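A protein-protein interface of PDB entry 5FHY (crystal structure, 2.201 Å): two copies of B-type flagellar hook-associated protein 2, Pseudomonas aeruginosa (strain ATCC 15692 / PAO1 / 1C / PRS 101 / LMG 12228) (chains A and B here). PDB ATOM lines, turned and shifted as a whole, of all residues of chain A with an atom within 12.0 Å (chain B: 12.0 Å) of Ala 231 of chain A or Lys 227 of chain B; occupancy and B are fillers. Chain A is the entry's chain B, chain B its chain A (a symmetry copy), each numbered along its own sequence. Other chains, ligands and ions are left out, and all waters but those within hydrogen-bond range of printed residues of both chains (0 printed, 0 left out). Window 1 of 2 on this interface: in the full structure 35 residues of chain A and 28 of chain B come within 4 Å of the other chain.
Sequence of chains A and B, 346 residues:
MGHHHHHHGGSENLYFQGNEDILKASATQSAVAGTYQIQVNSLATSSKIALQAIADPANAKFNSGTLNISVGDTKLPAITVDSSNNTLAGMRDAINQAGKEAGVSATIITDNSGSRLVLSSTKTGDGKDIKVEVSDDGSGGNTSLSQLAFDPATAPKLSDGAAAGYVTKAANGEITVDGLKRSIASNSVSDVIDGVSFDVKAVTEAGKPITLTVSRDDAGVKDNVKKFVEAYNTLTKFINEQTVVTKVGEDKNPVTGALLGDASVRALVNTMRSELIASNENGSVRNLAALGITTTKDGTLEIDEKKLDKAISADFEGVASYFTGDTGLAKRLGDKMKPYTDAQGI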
ATOM      1  N   LYS A 222      25.375  33.741 -11.619  1.00  0.00           N
ATOM      2  CA  LYS A 222      24.390  33.547 -10.554  1.00  0.00           C
ATOM      3  C   LYS A 222      23.207  32.602 -10.799  1.00  0.00           C
ATOM      4  O   LYS A 222      22.515  32.246  -9.845  1.00  0.00           O
ATOM      5  CB  LYS A 222      23.826  34.916 -10.157  1.00  0.00           C
ATOM      6  N   ASP A 223      22.947  32.196 -12.037  1.00  0.00           N
ATOM      7  CA  ASP A 223      21.901  31.193 -12.253  1.00  0.00           C
ATOM      8  C   ASP A 223      22.319  29.813 -11.739  1.00  0.00           C
ATOM      9  O   ASP A 223      21.617  29.202 -10.933  1.00  0.00           O
ATOM     10  CB  ASP A 223      21.532  31.105 -13.733  1.00  0.00           C
ATOM     11  N   ASN A 224      23.458  29.319 -12.220  1.00  0.00           N
ATOM     12  CA  ASN A 224      24.029  28.067 -11.725  1.00  0.00           C
ATOM     13  C   ASN A 224      24.622  28.189 -10.328  1.00  0.00           C
ATOM     14  O   ASN A 224      24.873  27.184  -9.663  1.00  0.00           O
ATOM     15  CB  ASN A 224      25.110  27.554 -12.676  1.00  0.00           C
ATOM     16  N   VAL A 225      24.849  29.423  -9.888  1.00  0.00           N
ATOM     17  CA  VAL A 225      25.385  29.671  -8.554  1.00  0.00           C
ATOM     18  C   VAL A 225      24.366  29.344  -7.470  1.00  0.00           C
ATOM     19  O   VAL A 225      24.733  29.078  -6.325  1.00  0.00           O
ATOM     20  CB  VAL A 225      25.845  31.128  -8.389  1.00  0.00           C
ATOM     21  N   LYS A 226      23.085  29.372  -7.831  1.00  0.00           N
ATOM     22  CA  LYS A 226      22.019  29.054  -6.886  1.00  0.00           C
ATOM     23  C   LYS A 226      22.080  27.587  -6.458  1.00  0.00           C
ATOM     24  O   LYS A 226      21.460  27.191  -5.471  1.00  0.00           O
ATOM     25  CB  LYS A 226      20.652  29.365  -7.496  1.00  0.00           C
ATOM     26  N   LYS A 227      22.822  26.786  -7.218  1.00  0.00           N
ATOM     27  CA  LYS A 227      23.061  25.383  -6.892  1.00  0.00           C
ATOM     28  C   LYS A 227      23.878  25.257  -5.612  1.00  0.00           C
ATOM     29  O   LYS A 227      23.396  24.771  -4.590  1.00  0.00           O
ATOM     30  CB  LYS A 227      23.772  24.669  -8.041  1.00  0.00           C
ATOM     31  N   PHE A 228      25.135  25.680  -5.695  1.00  0.00           N
ATOM     32  CA  PHE A 228      26.079  25.572  -4.587  1.00  0.00           C
ATOM     33  C   PHE A 228      25.693  26.414  -3.365  1.00  0.00           C
ATOM     34  O   PHE A 228      26.398  26.408  -2.358  1.00  0.00           O
ATOM     35  CB  PHE A 228      27.481  25.958  -5.059  1.00  0.00           C
ATOM     36  CG  PHE A 228      28.143  24.917  -5.921  1.00  0.00           C
ATOM     37  CD1 PHE A 228      27.651  24.619  -7.181  1.00  0.00           C
ATOM     38  CD2 PHE A 228      29.271  24.250  -5.475  1.00  0.00           C
ATOM     39  CE1 PHE A 228      28.265  23.666  -7.971  1.00  0.00           C
ATOM     40  CE2 PHE A 228      29.890  23.301  -6.262  1.00  0.00           C
ATOM     41  CZ  PHE A 228      29.390  23.011  -7.511  1.00  0.00           C
ATOM     42  N   VAL A 229      24.604  27.168  -3.470  1.00  0.00           N
ATOM     43  CA  VAL A 229      23.998  27.798  -2.302  1.00  0.00           C
ATOM     44  C   VAL A 229      23.174  26.742  -1.582  1.00  0.00           C
ATOM     45  O   VAL A 229      23.104  26.719  -0.354  1.00  0.00           O
ATOM     46  CB  VAL A 229      23.106  28.996  -2.669  1.00  0.00           C
ATOM     47  N   GLU A 230      22.537  25.883  -2.375  1.00  0.00           N
ATOM     48  CA  GLU A 230      21.717  24.788  -1.865  1.00  0.00           C
ATOM     49  C   GLU A 230      22.575  23.577  -1.509  1.00  0.00           C
ATOM     50  O   GLU A 230      22.491  23.078  -0.392  1.00  0.00           O
ATOM     51  CB  GLU A 230      20.650  24.395  -2.886  1.00  0.00           C
ATOM     52  N   ALA A 231      23.371  23.096  -2.467  1.00  0.00           N
ATOM     53  CA  ALA A 231      24.248  21.936  -2.263  1.00  0.00           C
ATOM     54  C   ALA A 231      25.007  22.104  -0.949  1.00  0.00           C
ATOM     55  O   ALA A 231      25.238  21.144  -0.213  1.00  0.00           O
ATOM     56  CB  ALA A 231      25.207  21.766  -3.430  1.00  0.00           C
ATOM     57  N   TYR A 232      25.401  23.346  -0.685  1.00  0.00           N
ATOM     58  CA  TYR A 232      25.914  23.762   0.612  1.00  0.00           C
ATOM     59  C   TYR A 232      24.831  23.640   1.683  1.00  0.00           C
ATOM     60  O   TYR A 232      24.982  22.887   2.646  1.00  0.00           O
ATOM     61  CB  TYR A 232      26.428  25.200   0.519  1.00  0.00           C
ATOM     62  CG  TYR A 232      26.471  25.964   1.821  1.00  0.00           C
ATOM     63  CD1 TYR A 232      27.518  25.808   2.720  1.00  0.00           C
ATOM     64  CD2 TYR A 232      25.467  26.874   2.134  1.00  0.00           C
ATOM     65  CE1 TYR A 232      27.548  26.525   3.905  1.00  0.00           C
ATOM     66  CE2 TYR A 232      25.487  27.588   3.309  1.00  0.00           C
ATOM     67  CZ  TYR A 232      26.529  27.413   4.192  1.00  0.00           C
ATOM     68  OH  TYR A 232      26.545  28.133   5.366  1.00  0.00           O
ATOM     69  N   ASN A 233      23.746  24.395   1.515  1.00  0.00           N
ATOM     70  CA  ASN A 233      22.675  24.464   2.507  1.00  0.00           C
ATOM     71  C   ASN A 233      21.997  23.112   2.712  1.00  0.00           C
ATOM     72  O   ASN A 233      21.499  22.818   3.796  1.00  0.00           O
ATOM     73  CB  ASN A 233      21.631  25.510   2.109  1.00  0.00           C
ATOM     74  N   THR A 234      21.964  22.302   1.657  1.00  0.00           N
ATOM     75  CA  THR A 234      21.400  20.957   1.734  1.00  0.00           C
ATOM     76  C   THR A 234      22.266  20.055   2.600  1.00  0.00           C
ATOM     77  O   THR A 234      21.778  19.083   3.177  1.00  0.00           O
ATOM     78  CB  THR A 234      21.241  20.315   0.342  1.00  0.00           C
ATOM     79  N   LEU A 235      23.557  20.365   2.672  1.00  0.00           N
ATOM     80  CA  LEU A 235      24.466  19.593   3.508  1.00  0.00           C
ATOM     81  C   LEU A 235      24.562  20.235   4.891  1.00  0.00           C
ATOM     82  O   LEU A 235      25.647  20.388   5.453  1.00  0.00           O
ATOM     83  CB  LEU A 235      25.846  19.484   2.860  1.00  0.00           C
ATOM     84  CG  LEU A 235      26.091  18.128   2.193  1.00  0.00           C
ATOM     85  CD1 LEU A 235      25.091  17.935   1.065  1.00  0.00           C
ATOM     86  CD2 LEU A 235      27.518  17.989   1.678  1.00  0.00           C
ATOM     87  N   THR A 236      23.407  20.636   5.413  1.00  0.00           N
ATOM     88  CA  THR A 236      23.290  21.120   6.782  1.00  0.00           C
ATOM     89  C   THR A 236      22.369  20.193   7.561  1.00  0.00           C
ATOM     90  O   THR A 236      22.622  19.884   8.724  1.00  0.00           O
ATOM     91  CB  THR A 236      22.744  22.557   6.844  1.00  0.00           C
ATOM     92  N   LYS A 237      21.292  19.767   6.910  1.00  0.00           N
ATOM     93  CA  LYS A 237      20.313  18.871   7.519  1.00  0.00           C
ATOM     94  C   LYS A 237      20.748  17.406   7.482  1.00  0.00           C
ATOM     95  O   LYS A 237      21.194  16.856   8.490  1.00  0.00           O
ATOM     96  CB  LYS A 237      18.955  19.024   6.829  1.00  0.00           C
ATOM     97  N   PHE A 238      20.616  16.779   6.315  1.00  0.00           N
ATOM     98  CA  PHE A 238      20.833  15.337   6.179  1.00  0.00           C
ATOM     99  C   PHE A 238      22.276  14.941   6.490  1.00  0.00           C
ATOM    100  O   PHE A 238      22.587  13.760   6.662  1.00  0.00           O
ATOM    101  CB  PHE A 238      20.453  14.869   4.776  1.00  0.00           C
ATOM    102  N   ILE A 239      23.148  15.941   6.541  1.00  0.00           N
ATOM    103  CA  ILE A 239      24.501  15.775   7.047  1.00  0.00           C
ATOM    104  C   ILE A 239      24.737  16.833   8.120  1.00  0.00           C
ATOM    105  O   ILE A 239      24.530  18.021   7.875  1.00  0.00           O
ATOM    106  CB  ILE A 239      25.556  15.898   5.935  1.00  0.00           C
ATOM    107  N   ASN A 240      25.145  16.372   9.304  1.00  0.00           N
ATOM    108  CA  ASN A 240      25.472  17.200  10.475  1.00  0.00           C
ATOM    109  C   ASN A 240      24.236  17.701  11.233  1.00  0.00           C
ATOM    110  O   ASN A 240      24.348  18.539  12.129  1.00  0.00           O
ATOM    111  CB  ASN A 240      26.357  18.390  10.084  1.00  0.00           C
ATOM    112  N   GLU A 241      23.063  17.188  10.870  1.00  0.00           N
ATOM    113  CA  GLU A 241      21.843  17.425  11.640  1.00  0.00           C
ATOM    114  C   GLU A 241      20.958  16.184  11.590  1.00  0.00           C
ATOM    115  O   GLU A 241      20.094  15.982  12.444  1.00  0.00           O
ATOM    116  CB  GLU A 241      21.082  18.645  11.121  1.00  0.00           C
ATOM    117  N   ALA B 219      20.561   6.649   5.514  1.00  0.00           N
ATOM    118  CA  ALA B 219      21.223   6.403   4.241  1.00  0.00           C
ATOM    119  C   ALA B 219      20.978   7.615   3.368  1.00  0.00           C
ATOM    120  O   ALA B 219      21.052   7.556   2.142  1.00  0.00           O
ATOM    121  CB  ALA B 219      20.708   5.137   3.587  1.00  0.00           C
ATOM    122  N   GLY B 220      20.698   8.724   4.044  1.00  0.00           N
ATOM    123  CA  GLY B 220      20.342   9.969   3.408  1.00  0.00           C
ATOM    124  C   GLY B 220      21.568  10.840   3.278  1.00  0.00           C
ATOM    125  O   GLY B 220      21.500  12.058   3.435  1.00  0.00           O
ATOM    126  N   VAL B 221      22.706  10.208   3.005  1.00  0.00           N
ATOM    127  CA  VAL B 221      23.827  10.947   2.461  1.00  0.00           C
ATOM    128  C   VAL B 221      23.644  10.858   0.953  1.00  0.00           C
ATOM    129  O   VAL B 221      24.490  11.296   0.170  1.00  0.00           O
ATOM    130  CB  VAL B 221      25.187  10.374   2.897  1.00  0.00           C
ATOM    131  N   LYS B 222      22.512  10.266   0.567  1.00  0.00           N
ATOM    132  CA  LYS B 222      22.069  10.206  -0.816  1.00  0.00           C
ATOM    133  C   LYS B 222      21.488  11.584  -1.105  1.00  0.00           C
ATOM    134  O   LYS B 222      21.256  11.968  -2.250  1.00  0.00           O
ATOM    135  CB  LYS B 222      21.044   9.093  -1.039  1.00  0.00           C
ATOM    136  N   ASP B 223      21.223  12.300  -0.015  1.00  0.00           N
ATOM    137  CA  ASP B 223      20.861  13.707  -0.035  1.00  0.00           C
ATOM    138  C   ASP B 223      22.100  14.474  -0.451  1.00  0.00           C
ATOM    139  O   ASP B 223      22.043  15.369  -1.286  1.00  0.00           O
ATOM    140  CB  ASP B 223      20.358  14.178   1.327  1.00  0.00           C
ATOM    141  CG  ASP B 223      20.366  15.689   1.458  1.00  0.00           C
ATOM    142  OD1 ASP B 223      19.390  16.335   1.023  1.00  0.00           O
ATOM    143  OD2 ASP B 223      21.357  16.230   1.997  1.00  0.00           O
ATOM    144  N   ASN B 224      23.219  14.134   0.182  1.00  0.00           N
ATOM    145  CA  ASN B 224      24.504  14.704  -0.193  1.00  0.00           C
ATOM    146  C   ASN B 224      24.926  14.238  -1.580  1.00  0.00           C
ATOM    147  O   ASN B 224      25.817  14.824  -2.195  1.00  0.00           O
ATOM    148  CB  ASN B 224      25.576  14.331   0.832  1.00  0.00           C
ATOM    149  N   VAL B 225      24.293  13.175  -2.067  1.00  0.00           N
ATOM    150  CA  VAL B 225      24.521  12.723  -3.434  1.00  0.00           C
ATOM    151  C   VAL B 225      23.853  13.705  -4.388  1.00  0.00           C
ATOM    152  O   VAL B 225      24.227  13.805  -5.556  1.00  0.00           O
ATOM    153  CB  VAL B 225      23.985  11.304  -3.684  1.00  0.00           C
ATOM    154  N   LYS B 226      22.835  14.404  -3.887  1.00  0.00           N
ATOM    155  CA  LYS B 226      22.136  15.418  -4.676  1.00  0.00           C
ATOM    156  C   LYS B 226      23.046  16.612  -4.948  1.00  0.00           C
ATOM    157  O   LYS B 226      22.732  17.457  -5.788  1.00  0.00           O
ATOM    158  CB  LYS B 226      20.852  15.877  -3.985  1.00  0.00           C
ATOM    159  N   LYS B 227      24.160  16.690  -4.222  1.00  0.00           N
ATOM    160  CA  LYS B 227      25.147  17.731  -4.469  1.00  0.00           C
ATOM    161  C   LYS B 227      25.681  17.506  -5.868  1.00  0.00           C
ATOM    162  O   LYS B 227      25.352  18.247  -6.786  1.00  0.00           O
ATOM    163  CB  LYS B 227      26.282  17.695  -3.443  1.00  0.00           C
ATOM    164  CG  LYS B 227      27.396  18.696  -3.722  1.00  0.00           C
ATOM    165  CD  LYS B 227      28.674  18.317  -2.995  1.00  0.00           C
ATOM    166  CE  LYS B 227      29.219  16.987  -3.498  1.00  0.00           C
ATOM    167  NZ  LYS B 227      29.548  17.026  -4.951  1.00  0.00           N
ATOM    168  N   PHE B 228      26.475  16.450  -6.032  1.00  0.00           N
ATOM    169  CA  PHE B 228      27.070  16.127  -7.325  1.00  0.00           C
ATOM    170  C   PHE B 228      26.006  15.717  -8.342  1.00  0.00           C
ATOM    171  O   PHE B 228      26.311  15.491  -9.509  1.00  0.00           O
ATOM    172  CB  PHE B 228      28.108  15.013  -7.180  1.00  0.00           C
ATOM    173  N   VAL B 229      24.757  15.605  -7.897  1.00  0.00           N
ATOM    174  CA  VAL B 229      23.642  15.469  -8.823  1.00  0.00           C
ATOM    175  C   VAL B 229      23.319  16.858  -9.335  1.00  0.00           C
ATOM    176  O   VAL B 229      22.996  17.043 -10.503  1.00  0.00           O
ATOM    177  CB  VAL B 229      22.401  14.839  -8.174  1.00  0.00           C
ATOM    178  N   GLU B 230      23.373  17.835  -8.435  1.00  0.00           N
ATOM    179  CA  GLU B 230      23.173  19.218  -8.827  1.00  0.00           C
ATOM    180  C   GLU B 230      24.505  19.812  -9.278  1.00  0.00           C
ATOM    181  O   GLU B 230      24.642  20.233 -10.419  1.00  0.00           O
ATOM    182  CB  GLU B 230      22.581  20.035  -7.678  1.00  0.00           C
ATOM    183  N   ALA B 231      25.495  19.785  -8.385  1.00  0.00           N
ATOM    184  CA  ALA B 231      26.808  20.391  -8.630  1.00  0.00           C
ATOM    185  C   ALA B 231      27.402  20.029  -9.986  1.00  0.00           C
ATOM    186  O   ALA B 231      27.968  20.882 -10.666  1.00  0.00           O
ATOM    187  CB  ALA B 231      27.779  19.998  -7.522  1.00  0.00           C
ATOM    188  N   TYR B 232      27.299  18.762 -10.370  1.00  0.00           N
ATOM    189  CA  TYR B 232      27.644  18.367 -11.730  1.00  0.00           C
ATOM    190  C   TYR B 232      26.630  18.909 -12.734  1.00  0.00           C
ATOM    191  O   TYR B 232      26.939  19.791 -13.536  1.00  0.00           O
ATOM    192  CB  TYR B 232      27.744  16.846 -11.854  1.00  0.00           C
ATOM    193  N   ASN B 233      25.418  18.357 -12.690  1.00  0.00           N
ATOM    194  CA  ASN B 233      24.390  18.654 -13.686  1.00  0.00           C
ATOM    195  C   ASN B 233      23.942  20.114 -13.738  1.00  0.00           C
ATOM    196  O   ASN B 233      23.575  20.604 -14.805  1.00  0.00           O
ATOM    197  CB  ASN B 233      23.166  17.763 -13.459  1.00  0.00           C
ATOM    198  N   THR B 234      23.941  20.810 -12.602  1.00  0.00           N
ATOM    199  CA  THR B 234      23.600  22.231 -12.627  1.00  0.00           C
ATOM    200  C   THR B 234      24.721  23.017 -13.292  1.00  0.00           C
ATOM    201  O   THR B 234      24.484  24.063 -13.896  1.00  0.00           O
ATOM    202  CB  THR B 234      23.340  22.808 -11.218  1.00  0.00           C
ATOM    203  N   LEU B 235      25.948  22.521 -13.158  1.00  0.00           N
ATOM    204  CA  LEU B 235      27.094  23.150 -13.805  1.00  0.00           C
ATOM    205  C   LEU B 235      27.416  22.476 -15.138  1.00  0.00           C
ATOM    206  O   LEU B 235      28.566  22.460 -15.578  1.00  0.00           O
ATOM    207  CB  LEU B 235      28.315  23.138 -12.886  1.00  0.00           C
ATOM    208  CG  LEU B 235      28.587  24.501 -12.241  1.00  0.00           C
ATOM    209  CD1 LEU B 235      27.423  24.917 -11.347  1.00  0.00           C
ATOM    210  CD2 LEU B 235      29.897  24.500 -11.468  1.00  0.00           C
ATOM    211  N   THR B 236      26.393  21.910 -15.768  1.00  0.00           N
ATOM    212  CA  THR B 236      26.519  21.375 -17.117  1.00  0.00           C
ATOM    213  C   THR B 236      25.611  22.198 -18.009  1.00  0.00           C
ATOM    214  O   THR B 236      25.817  22.299 -19.218  1.00  0.00           O
ATOM    215  CB  THR B 236      26.135  19.886 -17.200  1.00  0.00           C
ATOM    216  N   LYS B 237      24.591  22.774 -17.387  1.00  0.00           N
ATOM    217  CA  LYS B 237      23.641  23.625 -18.081  1.00  0.00           C
ATOM    218  C   LYS B 237      24.224  25.024 -18.244  1.00  0.00           C
ATOM    219  O   LYS B 237      24.718  25.381 -19.312  1.00  0.00           O
ATOM    220  CB  LYS B 237      22.313  23.683 -17.322  1.00  0.00           C
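O of Thr 234 of chain A lies close to OD2 of Asp 223 of chain B (3.1 Å).
Asn 224 of chain A touches Leu 235 of chain B, and with the chains exchanged Leu 235 of chain A touches Asn 224 of chain B.
Lys 227 of chain A touches Thr 234 of chain B, but with the chains exchanged Thr 234 of chain A does not touch Lys 227 of chain B (6.5 Å).
Ala 231 of chain A touches Lys 227 of chain B, but with the chains exchanged Lys 227 of chain A does not touch Ala 231 of chain B (5.2 Å).
Thr 234 of chain A touches Asp 223 of chain B, but with the chains exchanged Asp 223 of chain A does not touch Thr 234 of chain B (6.5 Å).
Positions printed for both chains: 222, 223, 224, 225, 226, 227, 228, 229, 230, 231, 232, 233, 234, 235, 236 and 237.
Hydrophobic or aromatic side chains of chain A that line the printed part of chain B: Phe 228, Ala 231, Leu 235 and Phe 238.
Among the printed residues, no Asp or Glu carboxylate lies within 4 Å of a Lys or Arg side-chain nitrogen of the other chain.
Of the printed residues of chain B, Ala 231 of chain A touches Lys 227 (3.8 Å).
Printed residues of chain A within 4 Å of Lys 227 of chain B: Ala 231.
Of chain B, only Thr 234 comes within 4 Å of Lys 227 of chain A.
Of chain B, only Ala 231 (3.4 Å) and Leu 235 (3.7 Å) come within 4 Å of Phe 228 of chain A.
No residue of chain B comes within 4 Å of Val 229 of chain A.
Asn 233 of chain A touches none of the printed residues of chain B.
Leu 235 of chain A touches just one residue of chain B: Asn 224.
Of chain A, only Thr 234 and Phe 238 come within 4 Å of Asp 223 of chain B.
No residue of chain A comes within 4 Å of Val 225 of chain B.
No residue of chain A comes within 4 Å of Lys 226 of chain B.
Phe 228 of chain B touches none of the printed residues of chain A.
No residue of chain A comes within 4 Å of Glu 230 of chain B.
No residue of chain A comes within 4 Å of Tyr 232 of chain B.
Of the printed residues of chain A, Gly 220 of chain B touches Phe 238 (3.3 Å).
Of the printed residues of chain B, Asn 224 of chain A touches Thr 234 (3.8 Å) and Leu 235 (3.8 Å).
Glu 241 of chain A touches none of the printed residues of chain B.
Tyr 232 of chain A touches none of the printed residues of chain B.
The nearest residue of chain B that does not touch Ala 231 of chain A is Ala 231 of chain B (5.1 Å).
The nearest residue of chain A that does not touch Lys 227 of chain B is Leu 235 of chain A (4.7 Å).
Among the printed residues, pairs that only touch across the chains: Phe 238 of chain A with Asp 223 of chain B, Phe 238 of chain A with Gly 220 of chain B, Phe 228 of chain A with Ala 231 of chain B, Leu 235 of chain A with Asn 224 of chain B, Phe 228 of chain A with Leu 235 of chain B, Lys 227 of chain A with Thr 234 of chain B, Asn 224 of chain A with Thr 234 of chain B, Asn 224 of chain A with Leu 235 of chain B and Ala 231 of chain A with Lys 227 of chain B.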
